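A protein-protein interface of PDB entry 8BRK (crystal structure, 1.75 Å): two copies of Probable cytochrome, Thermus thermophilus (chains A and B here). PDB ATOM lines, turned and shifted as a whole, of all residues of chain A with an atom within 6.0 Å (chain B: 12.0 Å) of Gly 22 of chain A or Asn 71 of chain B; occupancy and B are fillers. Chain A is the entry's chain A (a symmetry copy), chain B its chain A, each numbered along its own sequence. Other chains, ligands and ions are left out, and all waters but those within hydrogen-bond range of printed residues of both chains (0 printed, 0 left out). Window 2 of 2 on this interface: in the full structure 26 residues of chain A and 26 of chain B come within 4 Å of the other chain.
The backbone carbonyl oxygen (O) of Asn 71 of chain B lies within hydrogen-bond range of the backbone NH (N) of Lys 20 of chain A (2.7 Å). The backbone carbonyl oxygen (O) of Pro 21 of chain A lies close to the side-chain amide oxygen (OD1) of Asn 71 of chain B (3.3 Å). The backbone carbonyl oxygen (O) of Glu 18 of chain A sits at hydrogen-bond distance from the backbone NH (N) of Leu 73 of chain B, 2.8 Å away.
The side-chain amino group (NZ) of Lys 20 of chain A is in salt-bridge range of the side-chain carboxylate (OE1) of Glu 18 of chain A (2.6 Å). N of Leu 25 of chain A sits at hydrogen-bond distance from ND1 of His 23 of chain A.
O of Glu 18 of chain A touches CA of Ala 72 of chain B (3.1 Å). C of Leu 19 of chain A touches O of Asn 71 of chain B, 3.7 Å away. C of Gly 22 of chain A touches ND2 of Asn 71 of chain B, at 3.5 Å. Asn 71 of chain B touches His 23 of chain A.
Of the printed residues of chain B, Gly 22 of chain A touches Asn 71. Asn 71 of chain B touches just these residues of chain A: Leu 19, Lys 20, Pro 21, Gly 22 and His 23. Of the printed residues of chain B, Glu 18 of chain A touches Ala 72 (3.1 Å) and Leu 73 (2.8 Å). Printed residues of chain B within 4 Å of Lys 20 of chain A: Asn 71 (2.7 Å). Printed residues of chain B within 4 Å of Pro 21 of chain A: Asn 71. Printed residues of chain B within 4 Å of His 23 of chain A: Asn 71. No residue of chain B comes within 4 Å of Pro 24 of chain A. No residue of chain B comes within 4 Å of Tyr 26 of chain A. Printed residues of chain A within 4 Å of Leu 73 of chain B: Glu 18. Of the printed residues of chain A, Ala 72 of chain B touches Glu 18. Gly 70 of chain B touches none of the printed residues of chain A. The nearest residue of chain B that does not touch Gly 22 of chain A is Gly 70 of chain B (7.3 Å). The nearest residue of chain A that does not touch Asn 71 of chain B is Glu 18 of chain A (4.3 Å). The nearest printed residue of chain A that does not touch Leu 73 of chain B is Lys 20 of chain A (4.1 Å).
Of the 12 printed residues of chain B, 3 touch a printed residue of chain A. Printed residues of chain B that touch a printed residue of chain A: Asn 71, Ala 72 and Leu 73. Hydrophobic or aromatic side chains of chain B that line the printed part of chain A: Ala 72 and Leu 73. Of the 9 printed residues of chain A, 6 touch a printed residue of chain B. Among the printed residues, 7 pairs touch across the chains. Among the printed residues, no Asp or Glu carboxylate lies within 4 Å of a Lys or Arg side-chain nitrogen of the other chain.
2 positions are printed for both chains. Of the 7 pairs that touch across the chains among the printed residues, none has its exchanged pair printed and touching as well.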
ATOM      1  N   GLU A  18     -26.458   6.297 -20.181  1.00  0.00           N
ATOM      2  CA  GLU A  18     -26.150   5.211 -21.135  1.00  0.00           C
ATOM      3  C   GLU A  18     -26.813   3.951 -20.601  1.00  0.00           C
ATOM      4  O   GLU A  18     -26.652   3.665 -19.435  1.00  0.00           O
ATOM      5  CB  GLU A  18     -24.657   5.017 -21.365  1.00  0.00           C
ATOM      6  CG  GLU A  18     -24.381   4.012 -22.471  1.00  0.00           C
ATOM      7  CD  GLU A  18     -23.173   3.129 -22.261  1.00  0.00           C
ATOM      8  OE1 GLU A  18     -22.507   3.284 -21.222  1.00  0.00           O
ATOM      9  OE2 GLU A  18     -22.905   2.311 -23.155  1.00  0.00           O
ATOM     10  N   LEU A  19     -27.588   3.297 -21.437  1.00  0.00           N
ATOM     11  CA  LEU A  19     -28.158   1.970 -21.144  1.00  0.00           C
ATOM     12  C   LEU A  19     -27.275   0.920 -21.814  1.00  0.00           C
ATOM     13  O   LEU A  19     -27.116   0.972 -23.018  1.00  0.00           O
ATOM     14  CB  LEU A  19     -29.602   1.914 -21.658  1.00  0.00           C
ATOM     15  CG  LEU A  19     -30.547   2.933 -21.031  1.00  0.00           C
ATOM     16  CD1 LEU A  19     -31.970   2.678 -21.479  1.00  0.00           C
ATOM     17  CD2 LEU A  19     -30.434   2.893 -19.523  1.00  0.00           C
ATOM     18  N   LYS A  20     -26.711   0.029 -21.016  1.00  0.00           N
ATOM     19  CA  LYS A  20     -25.730  -0.984 -21.473  1.00  0.00           C
ATOM     20  C   LYS A  20     -26.476  -2.301 -21.673  1.00  0.00           C
ATOM     21  O   LYS A  20     -27.609  -2.490 -21.189  1.00  0.00           O
ATOM     22  CB  LYS A  20     -24.615  -1.150 -20.442  1.00  0.00           C
ATOM     23  CG  LYS A  20     -23.860   0.110 -20.055  1.00  0.00           C
ATOM     24  CD  LYS A  20     -22.922  -0.157 -18.897  1.00  0.00           C
ATOM     25  CE  LYS A  20     -21.997   0.990 -18.534  1.00  0.00           C
ATOM     26  NZ  LYS A  20     -21.292   1.515 -19.728  1.00  0.00           N
ATOM     27  N   PRO A  21     -25.858  -3.242 -22.416  1.00  0.00           N
ATOM     28  CA  PRO A  21     -26.459  -4.560 -22.642  1.00  0.00           C
ATOM     29  C   PRO A  21     -26.908  -5.233 -21.337  1.00  0.00           C
ATOM     30  O   PRO A  21     -26.209  -5.177 -20.345  1.00  0.00           O
ATOM     31  CB  PRO A  21     -25.317  -5.313 -23.332  1.00  0.00           C
ATOM     32  CG  PRO A  21     -24.589  -4.226 -24.087  1.00  0.00           C
ATOM     33  CD  PRO A  21     -24.582  -3.056 -23.129  1.00  0.00           C
ATOM     34  N   GLY A  22     -28.109  -5.797 -21.348  1.00  0.00           N
ATOM     35  CA  GLY A  22     -28.718  -6.442 -20.176  1.00  0.00           C
ATOM     36  C   GLY A  22     -29.675  -5.514 -19.461  1.00  0.00           C
ATOM     37  O   GLY A  22     -30.519  -6.010 -18.697  1.00  0.00           O
ATOM     38  N   HIS A  23     -29.572  -4.203 -19.687  1.00  0.00           N
ATOM     39  CA  HIS A  23     -30.583  -3.262 -19.163  1.00  0.00           C
ATOM     40  C   HIS A  23     -31.936  -3.667 -19.746  1.00  0.00           C
ATOM     41  O   HIS A  23     -32.022  -4.010 -20.928  1.00  0.00           O
ATOM     42  CB  HIS A  23     -30.223  -1.814 -19.472  1.00  0.00           C
ATOM     43  CG  HIS A  23     -31.049  -0.873 -18.669  1.00  0.00           C
ATOM     44  ND1 HIS A  23     -32.347  -0.526 -19.044  1.00  0.00           N
ATOM     45  CD2 HIS A  23     -30.788  -0.249 -17.507  1.00  0.00           C
ATOM     46  CE1 HIS A  23     -32.843   0.288 -18.141  1.00  0.00           C
ATOM     47  NE2 HIS A  23     -31.897   0.486 -17.189  1.00  0.00           N
ATOM     48  N   PRO A  24     -33.014  -3.663 -18.930  1.00  0.00           N
ATOM     49  CA  PRO A  24     -34.328  -4.069 -19.406  1.00  0.00           C
ATOM     50  C   PRO A  24     -34.822  -3.232 -20.591  1.00  0.00           C
ATOM     51  O   PRO A  24     -35.615  -3.748 -21.316  1.00  0.00           O
ATOM     52  CB  PRO A  24     -35.275  -3.900 -18.212  1.00  0.00           C
ATOM     53  CG  PRO A  24     -34.451  -3.296 -17.091  1.00  0.00           C
ATOM     54  CD  PRO A  24     -32.997  -3.373 -17.488  1.00  0.00           C
ATOM     55  N   LEU A  25     -34.348  -1.998 -20.763  1.00  0.00           N
ATOM     56  CA  LEU A  25     -34.751  -1.124 -21.905  1.00  0.00           C
ATOM     57  C   LEU A  25     -33.703  -1.167 -23.017  1.00  0.00           C
ATOM     58  O   LEU A  25     -33.787  -0.317 -23.912  1.00  0.00           O
ATOM     59  CB  LEU A  25     -34.907   0.313 -21.401  1.00  0.00           C
ATOM     60  CG  LEU A  25     -36.088   0.550 -20.470  1.00  0.00           C
ATOM     61  CD1 LEU A  25     -36.174   2.010 -20.097  1.00  0.00           C
ATOM     62  CD2 LEU A  25     -37.378   0.119 -21.134  1.00  0.00           C
ATOM     63  N   TYR A  26     -32.725  -2.070 -22.943  1.00  0.00           N
ATOM     64  CA  TYR A  26     -31.579  -2.087 -23.885  1.00  0.00           C
ATOM     65  C   TYR A  26     -32.055  -2.350 -25.323  1.00  0.00           C
ATOM     66  O   TYR A  26     -31.588  -1.653 -26.239  1.00  0.00           O
ATOM     67  CB  TYR A  26     -30.491  -3.070 -23.465  1.00  0.00           C
ATOM     68  CG  TYR A  26     -29.326  -2.953 -24.403  1.00  0.00           C
ATOM     69  CD1 TYR A  26     -28.469  -1.874 -24.306  1.00  0.00           C
ATOM     70  CD2 TYR A  26     -29.183  -3.812 -25.477  1.00  0.00           C
ATOM     71  CE1 TYR A  26     -27.419  -1.708 -25.182  1.00  0.00           C
ATOM     72  CE2 TYR A  26     -28.135  -3.662 -26.367  1.00  0.00           C
ATOM     73  CZ  TYR A  26     -27.255  -2.605 -26.219  1.00  0.00           C
ATOM     74  OH  TYR A  26     -26.224  -2.414 -27.081  1.00  0.00           O
ATOM     75  N   GLU B  18     -17.059  10.173 -22.344  1.00  0.00           N
ATOM     76  CA  GLU B  18     -16.604   9.592 -21.064  1.00  0.00           C
ATOM     77  C   GLU B  18     -15.163   9.152 -21.264  1.00  0.00           C
ATOM     78  O   GLU B  18     -14.893   8.495 -22.246  1.00  0.00           O
ATOM     79  CB  GLU B  18     -17.486   8.453 -20.573  1.00  0.00           C
ATOM     80  CG  GLU B  18     -17.092   7.991 -19.180  1.00  0.00           C
ATOM     81  CD  GLU B  18     -17.217   6.507 -18.926  1.00  0.00           C
ATOM     82  OE1 GLU B  18     -17.624   5.786 -19.854  1.00  0.00           O
ATOM     83  OE2 GLU B  18     -16.923   6.098 -17.792  1.00  0.00           O
ATOM     84  N   LYS B  20     -12.414   6.842 -19.630  1.00  0.00           N
ATOM     85  CA  LYS B  20     -12.388   5.655 -18.742  1.00  0.00           C
ATOM     86  C   LYS B  20     -10.955   5.471 -18.249  1.00  0.00           C
ATOM     87  O   LYS B  20      -9.994   6.036 -18.806  1.00  0.00           O
ATOM     88  CB  LYS B  20     -12.859   4.414 -19.498  1.00  0.00           C
ATOM     89  CG  LYS B  20     -14.230   4.498 -20.148  1.00  0.00           C
ATOM     90  CD  LYS B  20     -14.490   3.286 -21.016  1.00  0.00           C
ATOM     91  CE  LYS B  20     -15.894   3.185 -21.584  1.00  0.00           C
ATOM     92  NZ  LYS B  20     -16.920   3.359 -20.527  1.00  0.00           N
ATOM     93  N   ALA B  66     -18.500   9.381 -13.426  1.00  0.00           N
ATOM     94  CA  ALA B  66     -19.299   8.391 -14.167  1.00  0.00           C
ATOM     95  C   ALA B  66     -19.577   7.283 -13.161  1.00  0.00           C
ATOM     96  O   ALA B  66     -18.603   6.839 -12.539  1.00  0.00           O
ATOM     97  CB  ALA B  66     -18.537   7.920 -15.367  1.00  0.00           C
ATOM     98  N   LYS B  67     -20.844   6.990 -12.900  1.00  0.00           N
ATOM     99  CA  LYS B  67     -21.286   5.915 -11.983  1.00  0.00           C
ATOM    100  C   LYS B  67     -21.868   4.795 -12.838  1.00  0.00           C
ATOM    101  O   LYS B  67     -22.792   5.073 -13.577  1.00  0.00           O
ATOM    102  CB  LYS B  67     -22.306   6.480 -10.993  1.00  0.00           C
ATOM    103  CG  LYS B  67     -21.747   7.527 -10.042  1.00  0.00           C
ATOM    104  CD  LYS B  67     -22.803   8.116  -9.132  1.00  0.00           C
ATOM    105  CE  LYS B  67     -23.432   7.108  -8.192  1.00  0.00           C
ATOM    106  NZ  LYS B  67     -24.903   7.276  -8.139  1.00  0.00           N
ATOM    107  N   VAL B  68     -21.281   3.599 -12.816  1.00  0.00           N
ATOM    108  CA  VAL B  68     -21.905   2.393 -13.432  1.00  0.00           C
ATOM    109  C   VAL B  68     -22.757   1.726 -12.338  1.00  0.00           C
ATOM    110  O   VAL B  68     -22.217   1.367 -11.290  1.00  0.00           O
ATOM    111  CB  VAL B  68     -20.841   1.474 -14.058  1.00  0.00           C
ATOM    112  CG1 VAL B  68     -21.445   0.167 -14.562  1.00  0.00           C
ATOM    113  CG2 VAL B  68     -20.092   2.186 -15.183  1.00  0.00           C
ATOM    114  N   GLU B  69     -24.077   1.706 -12.500  1.00  0.00           N
ATOM    115  CA  GLU B  69     -25.017   1.050 -11.550  1.00  0.00           C
ATOM    116  C   GLU B  69     -25.971   0.206 -12.379  1.00  0.00           C
ATOM    117  O   GLU B  69     -26.571   0.743 -13.311  1.00  0.00           O
ATOM    118  CB  GLU B  69     -25.900   2.012 -10.755  1.00  0.00           C
ATOM    119  CG  GLU B  69     -25.259   2.670  -9.541  1.00  0.00           C
ATOM    120  CD  GLU B  69     -26.266   3.395  -8.648  1.00  0.00           C
ATOM    121  OE1 GLU B  69     -27.486   3.375  -8.978  1.00  0.00           O
ATOM    122  OE2 GLU B  69     -25.845   3.966  -7.603  1.00  0.00           O
ATOM    123  N   GLY B  70     -26.141  -1.048 -12.004  1.00  0.00           N
ATOM    124  CA  GLY B  70     -26.691  -2.061 -12.906  1.00  0.00           C
ATOM    125  C   GLY B  70     -25.958  -2.027 -14.232  1.00  0.00           C
ATOM    126  O   GLY B  70     -24.690  -2.041 -14.268  1.00  0.00           O
ATOM    127  N   ASN B  71     -26.743  -1.957 -15.286  1.00  0.00           N
ATOM    128  CA  ASN B  71     -26.296  -1.941 -16.697  1.00  0.00           C
ATOM    129  C   ASN B  71     -26.552  -0.537 -17.251  1.00  0.00           C
ATOM    130  O   ASN B  71     -27.124  -0.427 -18.338  1.00  0.00           O
ATOM    131  CB  ASN B  71     -27.066  -2.997 -17.482  1.00  0.00           C
ATOM    132  CG  ASN B  71     -26.583  -4.378 -17.113  1.00  0.00           C
ATOM    133  OD1 ASN B  71     -25.387  -4.646 -17.158  1.00  0.00           O
ATOM    134  ND2 ASN B  71     -27.494  -5.231 -16.715  1.00  0.00           N
ATOM    135  N   ALA B  72     -26.158   0.488 -16.501  1.00  0.00           N
ATOM    136  CA  ALA B  72     -26.366   1.885 -16.906  1.00  0.00           C
ATOM    137  C   ALA B  72     -25.127   2.664 -16.527  1.00  0.00           C
ATOM    138  O   ALA B  72     -24.531   2.352 -15.477  1.00  0.00           O
ATOM    139  CB  ALA B  72     -27.597   2.441 -16.237  1.00  0.00           C
ATOM    140  N   LEU B  73     -24.809   3.669 -17.324  1.00  0.00           N
ATOM    141  CA  LEU B  73     -23.904   4.767 -16.912  1.00  0.00           C
ATOM    142  C   LEU B  73     -24.775   5.952 -16.511  1.00  0.00           C
ATOM    143  O   LEU B  73     -25.574   6.439 -17.330  1.00  0.00           O
ATOM    144  CB  LEU B  73     -22.968   5.122 -18.070  1.00  0.00           C
ATOM    145  CG  LEU B  73     -22.096   6.373 -17.873  1.00  0.00           C
ATOM    146  CD1 LEU B  73     -21.165   6.238 -16.705  1.00  0.00           C
ATOM    147  CD2 LEU B  73     -21.288   6.659 -19.122  1.00  0.00           C
ATOM    148  N   LEU B  74     -24.587   6.393 -15.286  1.00  0.00           N
ATOM    149  CA  LEU B  74     -25.328   7.509 -14.681  1.00  0.00           C
ATOM    150  C   LEU B  74     -24.360   8.655 -14.448  1.00  0.00           C
ATOM    151  O   LEU B  74     -23.174   8.404 -14.174  1.00  0.00           O
ATOM    152  CB  LEU B  74     -25.956   7.052 -13.368  1.00  0.00           C
ATOM    153  CG  LEU B  74     -27.008   5.960 -13.520  1.00  0.00           C
ATOM    154  CD1 LEU B  74     -26.384   4.629 -13.210  1.00  0.00           C
ATOM    155  CD2 LEU B  74     -28.180   6.196 -12.590  1.00  0.00           C
ATOM    156  N   GLU B  75     -24.900   9.864 -14.463  1.00  0.00           N
ATOM    157  CA  GLU B  75     -24.165  11.072 -14.036  1.00  0.00           C
ATOM    158  C   GLU B  75     -24.003  11.085 -12.517  1.00  0.00           C
ATOM    159  O   GLU B  75     -24.973  11.076 -11.824  1.00  0.00           O
ATOM    160  CB  GLU B  75     -24.911  12.288 -14.555  1.00  0.00           C
ATOM    161  CG  GLU B  75     -25.075  12.208 -16.061  1.00  0.00           C
ATOM    162  CD  GLU B  75     -25.782  13.419 -16.600  1.00  0.00           C
ATOM    163  OE1 GLU B  75     -26.893  13.689 -16.098  1.00  0.00           O
ATOM    164  OE2 GLU B  75     -25.167  14.119 -17.430  1.00  0.00           O
